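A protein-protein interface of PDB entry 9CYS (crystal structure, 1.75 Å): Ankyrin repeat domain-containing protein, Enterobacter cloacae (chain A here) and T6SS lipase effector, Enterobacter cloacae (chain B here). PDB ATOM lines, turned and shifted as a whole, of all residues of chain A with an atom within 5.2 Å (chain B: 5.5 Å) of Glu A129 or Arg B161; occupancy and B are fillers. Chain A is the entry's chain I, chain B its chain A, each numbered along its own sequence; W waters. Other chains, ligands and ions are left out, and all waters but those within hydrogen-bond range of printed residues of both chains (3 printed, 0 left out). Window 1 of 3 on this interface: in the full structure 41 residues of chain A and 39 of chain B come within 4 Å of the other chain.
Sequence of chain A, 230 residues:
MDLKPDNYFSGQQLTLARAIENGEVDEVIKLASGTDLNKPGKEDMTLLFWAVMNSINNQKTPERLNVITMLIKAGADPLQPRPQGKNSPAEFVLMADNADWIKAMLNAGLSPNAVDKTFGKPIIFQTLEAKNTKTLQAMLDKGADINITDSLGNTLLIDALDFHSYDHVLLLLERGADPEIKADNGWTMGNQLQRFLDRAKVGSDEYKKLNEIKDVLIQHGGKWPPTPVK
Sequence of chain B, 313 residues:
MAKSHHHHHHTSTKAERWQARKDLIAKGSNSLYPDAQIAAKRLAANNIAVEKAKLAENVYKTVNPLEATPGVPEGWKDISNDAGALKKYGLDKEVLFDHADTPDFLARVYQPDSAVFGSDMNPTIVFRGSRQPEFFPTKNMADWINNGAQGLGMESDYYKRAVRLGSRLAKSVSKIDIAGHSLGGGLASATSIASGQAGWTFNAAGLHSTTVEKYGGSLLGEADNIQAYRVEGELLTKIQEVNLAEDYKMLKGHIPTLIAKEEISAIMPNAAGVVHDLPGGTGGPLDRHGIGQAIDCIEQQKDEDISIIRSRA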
ATOM      1  N   MET A  95     -11.689  22.374  17.977  1.00  0.00           N
ATOM      2  CA  MET A  95     -12.145  23.047  16.772  1.00  0.00           C
ATOM      3  C   MET A  95     -13.438  23.814  16.981  1.00  0.00           C
ATOM      4  O   MET A  95     -13.905  24.459  16.036  1.00  0.00           O
ATOM      5  CB  MET A  95     -12.309  22.012  15.651  1.00  0.00           C
ATOM      6  CG  MET A  95     -11.081  21.167  15.505  1.00  0.00           C
ATOM      7  SD  MET A  95     -11.330  19.935  14.217  1.00  0.00           S
ATOM      8  CE  MET A  95     -11.182  21.020  12.797  1.00  0.00           C
ATOM      9  N   PHE A 125      -2.409  22.719  18.263  1.00  0.00           N
ATOM     10  CA  PHE A 125      -2.440  23.134  16.861  1.00  0.00           C
ATOM     11  C   PHE A 125      -3.832  23.006  16.255  1.00  0.00           C
ATOM     12  O   PHE A 125      -4.152  23.720  15.296  1.00  0.00           O
ATOM     13  CB  PHE A 125      -1.416  22.328  16.059  1.00  0.00           C
ATOM     14  CG  PHE A 125      -0.005  22.846  16.208  1.00  0.00           C
ATOM     15  CD1 PHE A 125       0.465  23.877  15.392  1.00  0.00           C
ATOM     16  CD2 PHE A 125       0.824  22.351  17.195  1.00  0.00           C
ATOM     17  CE1 PHE A 125       1.758  24.372  15.553  1.00  0.00           C
ATOM     18  CE2 PHE A 125       2.120  22.847  17.368  1.00  0.00           C
ATOM     19  CZ  PHE A 125       2.578  23.857  16.541  1.00  0.00           C
ATOM     20  N   GLN A 126      -4.699  22.158  16.816  1.00  0.00           N
ATOM     21  CA  GLN A 126      -6.025  22.056  16.223  1.00  0.00           C
ATOM     22  C   GLN A 126      -6.888  23.284  16.491  1.00  0.00           C
ATOM     23  O   GLN A 126      -7.872  23.486  15.772  1.00  0.00           O
ATOM     24  CB  GLN A 126      -6.731  20.778  16.690  1.00  0.00           C
ATOM     25  CG  GLN A 126      -5.889  19.556  16.391  1.00  0.00           C
ATOM     26  CD  GLN A 126      -5.758  19.331  14.900  1.00  0.00           C
ATOM     27  OE1 GLN A 126      -6.751  19.323  14.164  1.00  0.00           O
ATOM     28  NE2 GLN A 126      -4.517  19.232  14.434  1.00  0.00           N
ATOM     29  N   THR A 127      -6.535  24.130  17.474  1.00  0.00           N
ATOM     30  CA  THR A 127      -7.308  25.351  17.694  1.00  0.00           C
ATOM     31  C   THR A 127      -7.256  26.295  16.501  1.00  0.00           C
ATOM     32  O   THR A 127      -8.125  27.165  16.372  1.00  0.00           O
ATOM     33  CB  THR A 127      -6.820  26.125  18.930  1.00  0.00           C
ATOM     34  OG1 THR A 127      -5.466  26.550  18.724  1.00  0.00           O
ATOM     35  CG2 THR A 127      -6.865  25.244  20.158  1.00  0.00           C
ATOM     36  N   LEU A 128      -6.248  26.158  15.636  1.00  0.00           N
ATOM     37  CA  LEU A 128      -6.083  27.133  14.568  1.00  0.00           C
ATOM     38  C   LEU A 128      -7.173  27.034  13.517  1.00  0.00           C
ATOM     39  O   LEU A 128      -7.313  27.956  12.713  1.00  0.00           O
ATOM     40  CB  LEU A 128      -4.708  26.969  13.923  1.00  0.00           C
ATOM     41  CG  LEU A 128      -3.543  27.122  14.896  1.00  0.00           C
ATOM     42  CD1 LEU A 128      -2.194  27.068  14.143  1.00  0.00           C
ATOM     43  CD2 LEU A 128      -3.648  28.416  15.712  1.00  0.00           C
ATOM     44  N   GLU A 129      -7.957  25.962  13.516  1.00  0.00           N
ATOM     45  CA  GLU A 129      -9.076  25.844  12.593  1.00  0.00           C
ATOM     46  C   GLU A 129     -10.391  26.302  13.196  1.00  0.00           C
ATOM     47  O   GLU A 129     -11.425  26.242  12.522  1.00  0.00           O
ATOM     48  CB  GLU A 129      -9.195  24.397  12.108  1.00  0.00           C
ATOM     49  CG  GLU A 129      -8.043  24.000  11.202  1.00  0.00           C
ATOM     50  CD  GLU A 129      -8.208  22.611  10.627  1.00  0.00           C
ATOM     51  OE1 GLU A 129      -9.074  22.431   9.743  1.00  0.00           O
ATOM     52  OE2 GLU A 129      -7.469  21.707  11.070  1.00  0.00           O
ATOM     53  N   ALA A 130     -10.378  26.770  14.435  1.00  0.00           N
ATOM     54  CA  ALA A 130     -11.599  27.241  15.057  1.00  0.00           C
ATOM     55  C   ALA A 130     -11.979  28.610  14.510  1.00  0.00           C
ATOM     56  O   ALA A 130     -11.139  29.383  14.033  1.00  0.00           O
ATOM     57  CB  ALA A 130     -11.449  27.294  16.578  1.00  0.00           C
ATOM     58  N   LYS A 131     -13.273  28.907  14.607  1.00  0.00           N
ATOM     59  CA  LYS A 131     -13.831  30.137  14.064  1.00  0.00           C
ATOM     60  C   LYS A 131     -13.361  31.369  14.834  1.00  0.00           C
ATOM     61  O   LYS A 131     -13.399  32.483  14.299  1.00  0.00           O
ATOM     62  CB  LYS A 131     -15.355  29.996  14.087  1.00  0.00           C
ATOM     63  CG  LYS A 131     -16.179  31.109  13.493  1.00  0.00           C
ATOM     64  CD  LYS A 131     -17.647  30.890  13.848  1.00  0.00           C
ATOM     65  CE  LYS A 131     -18.110  29.477  13.471  1.00  0.00           C
ATOM     66  NZ  LYS A 131     -17.921  29.135  12.028  1.00  0.00           N
ATOM     67  N   PHE A 163      -2.104  29.389   7.996  1.00  0.00           N
ATOM     68  CA  PHE A 163      -3.518  29.016   7.987  1.00  0.00           C
ATOM     69  C   PHE A 163      -4.426  30.191   7.642  1.00  0.00           C
ATOM     70  O   PHE A 163      -5.635  29.992   7.455  1.00  0.00           O
ATOM     71  CB  PHE A 163      -3.919  28.471   9.367  1.00  0.00           C
ATOM     72  CG  PHE A 163      -4.304  27.013   9.381  1.00  0.00           C
ATOM     73  CD1 PHE A 163      -5.215  26.509   8.474  1.00  0.00           C
ATOM     74  CD2 PHE A 163      -3.762  26.158  10.337  1.00  0.00           C
ATOM     75  CE1 PHE A 163      -5.578  25.164   8.507  1.00  0.00           C
ATOM     76  CE2 PHE A 163      -4.119  24.813  10.380  1.00  0.00           C
ATOM     77  CZ  PHE A 163      -5.024  24.318   9.460  1.00  0.00           C
ATOM     78  N   SER A 165      -5.191  32.278   9.830  1.00  0.00           N
ATOM     79  CA  SER A 165      -5.957  32.438  11.068  1.00  0.00           C
ATOM     80  C   SER A 165      -5.461  33.694  11.784  1.00  0.00           C
ATOM     81  O   SER A 165      -4.755  33.643  12.792  1.00  0.00           O
ATOM     82  CB  SER A 165      -5.810  31.199  11.935  1.00  0.00           C
ATOM     83  OG  SER A 165      -6.397  30.075  11.282  1.00  0.00           O
ATOM     84  N   GLU B  94       0.035  14.662   9.196  1.00  0.00           N
ATOM     85  CA  GLU B  94      -1.202  15.172   9.779  1.00  0.00           C
ATOM     86  C   GLU B  94      -1.861  16.220   8.890  1.00  0.00           C
ATOM     87  O   GLU B  94      -3.091  16.309   8.826  1.00  0.00           O
ATOM     88  CB  GLU B  94      -0.887  15.744  11.170  1.00  0.00           C
ATOM     89  CG  GLU B  94      -2.112  16.103  12.006  1.00  0.00           C
ATOM     90  CD  GLU B  94      -2.704  17.459  11.678  1.00  0.00           C
ATOM     91  OE1 GLU B  94      -1.958  18.371  11.244  1.00  0.00           O
ATOM     92  OE2 GLU B  94      -3.924  17.623  11.870  1.00  0.00           O
ATOM     93  N   VAL B  95      -1.061  17.035   8.191  1.00  0.00           N
ATOM     94  CA  VAL B  95      -1.638  18.141   7.431  1.00  0.00           C
ATOM     95  C   VAL B  95      -2.249  17.692   6.110  1.00  0.00           C
ATOM     96  O   VAL B  95      -2.867  18.515   5.430  1.00  0.00           O
ATOM     97  CB  VAL B  95      -0.578  19.230   7.162  1.00  0.00           C
ATOM     98  CG1 VAL B  95       0.001  19.776   8.484  1.00  0.00           C
ATOM     99  CG2 VAL B  95       0.544  18.682   6.274  1.00  0.00           C
ATOM    100  N   LEU B  96      -2.130  16.412   5.744  1.00  0.00           N
ATOM    101  CA  LEU B  96      -2.556  15.922   4.431  1.00  0.00           C
ATOM    102  C   LEU B  96      -4.037  15.559   4.359  1.00  0.00           C
ATOM    103  O   LEU B  96      -4.540  15.292   3.263  1.00  0.00           O
ATOM    104  CB  LEU B  96      -1.711  14.713   4.013  1.00  0.00           C
ATOM    105  CG  LEU B  96      -0.208  14.951   3.808  1.00  0.00           C
ATOM    106  CD1 LEU B  96       0.501  13.667   3.391  1.00  0.00           C
ATOM    107  CD2 LEU B  96       0.085  16.081   2.814  1.00  0.00           C
ATOM    108  N   PHE B  97      -4.767  15.555   5.476  1.00  0.00           N
ATOM    109  CA  PHE B  97      -6.194  15.292   5.351  1.00  0.00           C
ATOM    110  C   PHE B  97      -6.930  15.869   6.557  1.00  0.00           C
ATOM    111  O   PHE B  97      -6.318  16.269   7.548  1.00  0.00           O
ATOM    112  CB  PHE B  97      -6.506  13.796   5.164  1.00  0.00           C
ATOM    113  CG  PHE B  97      -5.957  12.845   6.235  1.00  0.00           C
ATOM    114  CD1 PHE B  97      -4.596  12.586   6.373  1.00  0.00           C
ATOM    115  CD2 PHE B  97      -6.846  12.147   7.054  1.00  0.00           C
ATOM    116  CE1 PHE B  97      -4.128  11.673   7.316  1.00  0.00           C
ATOM    117  CE2 PHE B  97      -6.391  11.229   7.991  1.00  0.00           C
ATOM    118  CZ  PHE B  97      -5.037  10.995   8.133  1.00  0.00           C
ATOM    119  N   ASP B  98      -8.246  15.985   6.410  1.00  0.00           N
ATOM    120  CA  ASP B  98      -9.083  16.391   7.528  1.00  0.00           C
ATOM    121  C   ASP B  98      -9.326  15.185   8.433  1.00  0.00           C
ATOM    122  O   ASP B  98      -9.287  14.034   8.001  1.00  0.00           O
ATOM    123  CB  ASP B  98     -10.386  17.008   6.997  1.00  0.00           C
ATOM    124  CG  ASP B  98     -11.629  16.536   7.732  1.00  0.00           C
ATOM    125  OD1 ASP B  98     -11.670  16.621   8.977  1.00  0.00           O
ATOM    126  OD2 ASP B  98     -12.576  16.091   7.050  1.00  0.00           O
ATOM    127  N   HIS B  99      -9.550  15.463   9.725  1.00  0.00           N
ATOM    128  CA  HIS B  99      -9.621  14.391  10.708  1.00  0.00           C
ATOM    129  C   HIS B  99     -10.914  14.310  11.502  1.00  0.00           C
ATOM    130  O   HIS B  99     -11.068  13.350  12.265  1.00  0.00           O
ATOM    131  CB  HIS B  99      -8.449  14.492  11.701  1.00  0.00           C
ATOM    132  CG  HIS B  99      -7.119  14.560  11.030  1.00  0.00           C
ATOM    133  ND1 HIS B  99      -6.451  13.430  10.619  1.00  0.00           N
ATOM    134  CD2 HIS B  99      -6.349  15.612  10.660  1.00  0.00           C
ATOM    135  CE1 HIS B  99      -5.315  13.779  10.041  1.00  0.00           C
ATOM    136  NE2 HIS B  99      -5.233  15.097  10.041  1.00  0.00           N
ATOM    137  N   PHE B 105     -11.722  15.586   1.925  1.00  0.00           N
ATOM    138  CA  PHE B 105     -10.538  16.405   1.658  1.00  0.00           C
ATOM    139  C   PHE B 105      -9.294  15.611   2.034  1.00  0.00           C
ATOM    140  O   PHE B 105      -9.037  15.358   3.218  1.00  0.00           O
ATOM    141  CB  PHE B 105     -10.546  17.718   2.435  1.00  0.00           C
ATOM    142  CG  PHE B 105      -9.191  18.409   2.457  1.00  0.00           C
ATOM    143  CD1 PHE B 105      -8.830  19.278   1.441  1.00  0.00           C
ATOM    144  CD2 PHE B 105      -8.265  18.162   3.463  1.00  0.00           C
ATOM    145  CE1 PHE B 105      -7.593  19.895   1.433  1.00  0.00           C
ATOM    146  CE2 PHE B 105      -7.016  18.757   3.445  1.00  0.00           C
ATOM    147  CZ  PHE B 105      -6.683  19.636   2.434  1.00  0.00           C
ATOM    148  N   GLU B 155     -16.002  24.995  11.759  1.00  0.00           N
ATOM    149  CA  GLU B 155     -15.856  25.611  10.448  1.00  0.00           C
ATOM    150  C   GLU B 155     -15.721  24.517   9.396  1.00  0.00           C
ATOM    151  O   GLU B 155     -15.016  23.526   9.600  1.00  0.00           O
ATOM    152  CB  GLU B 155     -14.638  26.540  10.424  1.00  0.00           C
ATOM    153  CG  GLU B 155     -14.698  27.669   9.396  1.00  0.00           C
ATOM    154  CD  GLU B 155     -13.346  28.347   9.187  1.00  0.00           C
ATOM    155  OE1 GLU B 155     -12.909  29.106  10.084  1.00  0.00           O
ATOM    156  OE2 GLU B 155     -12.719  28.123   8.127  1.00  0.00           O
ATOM    157  N   ASP B 157     -14.563  24.074   5.638  1.00  0.00           N
ATOM    158  CA  ASP B 157     -13.876  24.745   4.534  1.00  0.00           C
ATOM    159  C   ASP B 157     -12.630  23.937   4.170  1.00  0.00           C
ATOM    160  O   ASP B 157     -11.594  24.067   4.829  1.00  0.00           O
ATOM    161  CB  ASP B 157     -13.516  26.173   4.909  1.00  0.00           C
ATOM    162  CG  ASP B 157     -13.133  27.008   3.713  1.00  0.00           C
ATOM    163  OD1 ASP B 157     -13.345  26.551   2.567  1.00  0.00           O
ATOM    164  OD2 ASP B 157     -12.627  28.125   3.921  1.00  0.00           O
ATOM    165  N   TYR B 158     -12.736  23.123   3.117  1.00  0.00           N
ATOM    166  CA  TYR B 158     -11.554  22.443   2.600  1.00  0.00           C
ATOM    167  C   TYR B 158     -10.530  23.438   2.076  1.00  0.00           C
ATOM    168  O   TYR B 158      -9.325  23.153   2.089  1.00  0.00           O
ATOM    169  CB  TYR B 158     -11.922  21.462   1.485  1.00  0.00           C
ATOM    170  CG  TYR B 158     -12.835  20.315   1.862  1.00  0.00           C
ATOM    171  CD1 TYR B 158     -13.232  20.098   3.180  1.00  0.00           C
ATOM    172  CD2 TYR B 158     -13.310  19.449   0.882  1.00  0.00           C
ATOM    173  CE1 TYR B 158     -14.080  19.034   3.508  1.00  0.00           C
ATOM    174  CE2 TYR B 158     -14.155  18.390   1.199  1.00  0.00           C
ATOM    175  CZ  TYR B 158     -14.536  18.184   2.510  1.00  0.00           C
ATOM    176  OH  TYR B 158     -15.378  17.129   2.810  1.00  0.00           O
ATOM    177  N   TYR B 159     -10.976  24.611   1.609  1.00  0.00           N
ATOM    178  CA  TYR B 159     -10.004  25.544   1.046  1.00  0.00           C
ATOM    179  C   TYR B 159      -9.074  26.112   2.103  1.00  0.00           C
ATOM    180  O   TYR B 159      -7.981  26.568   1.756  1.00  0.00           O
ATOM    181  CB  TYR B 159     -10.697  26.675   0.286  1.00  0.00           C
ATOM    182  CG  TYR B 159     -11.087  26.224  -1.104  1.00  0.00           C
ATOM    183  CD1 TYR B 159     -10.144  26.171  -2.123  1.00  0.00           C
ATOM    184  CD2 TYR B 159     -12.381  25.792  -1.382  1.00  0.00           C
ATOM    185  CE1 TYR B 159     -10.484  25.731  -3.386  1.00  0.00           C
ATOM    186  CE2 TYR B 159     -12.730  25.354  -2.648  1.00  0.00           C
ATOM    187  CZ  TYR B 159     -11.777  25.322  -3.646  1.00  0.00           C
ATOM    188  OH  TYR B 159     -12.118  24.878  -4.910  1.00  0.00           O
ATOM    189  N   LYS B 160      -9.464  26.080   3.382  1.00  0.00           N
ATOM    190  CA  LYS B 160      -8.547  26.557   4.411  1.00  0.00           C
ATOM    191  C   LYS B 160      -7.328  25.653   4.525  1.00  0.00           C
ATOM    192  O   LYS B 160      -6.198  26.145   4.625  1.00  0.00           O
ATOM    193  CB  LYS B 160      -9.251  26.677   5.762  1.00  0.00           C
ATOM    194  CG  LYS B 160      -8.477  27.602   6.714  1.00  0.00           C
ATOM    195  CD  LYS B 160      -9.195  27.812   8.023  1.00  0.00           C
ATOM    196  CE  LYS B 160      -8.264  28.432   9.057  1.00  0.00           C
ATOM    197  NZ  LYS B 160      -8.090  29.903   8.870  1.00  0.00           N
ATOM    198  N   ARG B 161      -7.531  24.334   4.514  1.00  0.00           N
ATOM    199  CA  ARG B 161      -6.393  23.431   4.620  1.00  0.00           C
ATOM    200  C   ARG B 161      -5.595  23.414   3.322  1.00  0.00           C
ATOM    201  O   ARG B 161      -4.374  23.219   3.352  1.00  0.00           O
ATOM    202  CB  ARG B 161      -6.874  22.029   5.004  1.00  0.00           C
ATOM    203  CG  ARG B 161      -6.941  21.799   6.546  1.00  0.00           C
ATOM    204  CD  ARG B 161      -6.541  20.381   7.008  1.00  0.00           C
ATOM    205  NE  ARG B 161      -6.662  20.234   8.460  1.00  0.00           N
ATOM    206  CZ  ARG B 161      -5.907  19.436   9.210  1.00  0.00           C
ATOM    207  NH1 ARG B 161      -5.002  18.638   8.676  1.00  0.00           N
ATOM    208  NH2 ARG B 161      -6.061  19.441  10.533  1.00  0.00           N
ATOM    209  N   ALA B 162      -6.259  23.634   2.185  1.00  0.00           N
ATOM    210  CA  ALA B 162      -5.538  23.684   0.913  1.00  0.00           C
ATOM    211  C   ALA B 162      -4.686  24.947   0.816  1.00  0.00           C
ATOM    212  O   ALA B 162      -3.546  24.899   0.336  1.00  0.00           O
ATOM    213  CB  ALA B 162      -6.521  23.613  -0.257  1.00  0.00           C
ATOM    214  N   VAL B 163      -5.211  26.086   1.276  1.00  0.00           N
ATOM    215  CA  VAL B 163      -4.410  27.309   1.268  1.00  0.00           C
ATOM    216  C   VAL B 163      -3.250  27.192   2.250  1.00  0.00           C
ATOM    217  O   VAL B 163      -2.133  27.658   1.981  1.00  0.00           O
ATOM    218  CB  VAL B 163      -5.296  28.533   1.571  1.00  0.00           C
ATOM    219  CG1 VAL B 163      -4.442  29.744   1.916  1.00  0.00           C
ATOM    220  CG2 VAL B 163      -6.194  28.845   0.383  1.00  0.00           C
ATOM    221  N   ARG B 164      -3.493  26.566   3.407  1.00  0.00           N
ATOM    222  CA  ARG B 164      -2.422  26.358   4.376  1.00  0.00           C
ATOM    223  C   ARG B 164      -1.270  25.568   3.767  1.00  0.00           C
ATOM    224  O   ARG B 164      -0.096  25.910   3.949  1.00  0.00           O
ATOM    225  CB  ARG B 164      -2.972  25.638   5.611  1.00  0.00           C
ATOM    226  CG  ARG B 164      -2.008  25.595   6.792  1.00  0.00           C
ATOM    227  CD  ARG B 164      -1.157  24.332   6.831  1.00  0.00           C
ATOM    228  NE  ARG B 164      -0.850  23.946   8.201  1.00  0.00           N
ATOM    229  CZ  ARG B 164      -1.516  23.038   8.902  1.00  0.00           C
ATOM    230  NH1 ARG B 164      -2.475  22.300   8.356  1.00  0.00           N
ATOM    231  NH2 ARG B 164      -1.207  22.857  10.184  1.00  0.00           N
ATOM    232  N   LEU B 165      -1.587  24.483   3.063  1.00  0.00           N
ATOM    233  CA  LEU B 165      -0.545  23.733   2.367  1.00  0.00           C
ATOM    234  C   LEU B 165       0.158  24.607   1.338  1.00  0.00           C
ATOM    235  O   LEU B 165       1.380  24.523   1.174  1.00  0.00           O
ATOM    236  CB  LEU B 165      -1.161  22.502   1.709  1.00  0.00           C
ATOM    237  CG  LEU B 165      -1.628  21.447   2.716  1.00  0.00           C
ATOM    238  CD1 LEU B 165      -2.274  20.285   2.004  1.00  0.00           C
ATOM    239  CD2 LEU B 165      -0.459  20.959   3.534  1.00  0.00           C
ATOM    240  N   GLY B 166      -0.590  25.494   0.677  1.00  0.00           N
ATOM    241  CA  GLY B 166       0.036  26.428  -0.247  1.00  0.00           C
ATOM    242  C   GLY B 166       1.028  27.347   0.438  1.00  0.00           C
ATOM    243  O   GLY B 166       2.139  27.565  -0.051  1.00  0.00           O
HETATM  244  O   HOH W   1     -13.555  24.576  13.189  1.00  0.00           O
HETATM  245  O   HOH W   2     -11.344  26.179   9.877  1.00  0.00           O
HETATM  246  O   HOH W   3      -9.635  29.588  11.737  1.00  0.00           O
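The side-chain amide nitrogen (NE2) of Gln A126 lies within hydrogen-bond range of the side-chain carboxylate (OE2) of Glu B94 (3.1 Å).
NH2 of Arg B161 is in salt-bridge range of OE2 of Glu A129, 2.7 Å away.
NZ of Lys B160 is in hydrogen-bond range of O of Phe A163.
NZ of Lys B160 is in hydrogen-bond range of OG of Ser A165, 3.0 Å away.
The side-chain hydroxyl of Ser A165 lies within hydrogen-bond range of the backbone carbonyl oxygen of Leu A128, 2.7 Å away.
NE2 of His B99 sits at hydrogen-bond distance from O of Glu B94 (2.7 Å).
OE2 of Glu B94 is in salt-bridge range of NH2 of Arg B161, at 3.1 Å.
NH1 of Arg B161 is in hydrogen-bond range of O of Phe B97.
Among the printed residues, merely in contact across the chains: Phe A163 with Arg B164 (3.4 Å), Gln A126 with Arg B161 (3.7 Å), Leu A128 with Lys B160 (3.8 Å) and Glu A129 with Glu B155 (3.8 Å).
Of the printed residues of chain B, Leu A128 touches Lys B160 (3.8 Å).
Of chain B, only Glu B155 (3.8 Å) and Arg B161 (2.7 Å) come within 4 Å of Glu A129.
Of the printed residues of chain B, Phe A163 touches Lys B160 (2.8 Å) and Arg B164 (3.4 Å).
Of the printed residues of chain A, Glu B155 touches Glu A129.
Arg B161 touches just these residues of chain A: Gln A126 (3.7 Å) and Glu A129 (2.7 Å).
The nearest printed residue of chain B that does not touch Glu A129 is Lys B160 (4.5 Å).
The nearest residue of chain A that does not touch Arg B161 is Phe A163 (4.1 Å).
The nearest printed residue of chain A that does not touch Arg B164 is Phe A125 (5.6 Å).
Of the 18 printed residues of chain B, 5 touch a printed residue of chain A.
Along chain B the printed residues that touch a printed residue of chain A span positions 94 to 164.
Water W2 lies within hydrogen-bond range of O of Glu A129 and OE2 of Glu B155.
Water W3 lies within hydrogen-bond range of the backbone carbonyl oxygen of Ala A130, the backbone carbonyl oxygen of Leu A128, the side-chain amino group of Lys B160 and the side-chain hydroxyl of Ser A165.
Water W1 lies within hydrogen-bond range of the backbone carbonyl oxygen of Glu A129, the backbone NH of Glu B155 and the backbone carbonyl oxygen of Met A95.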
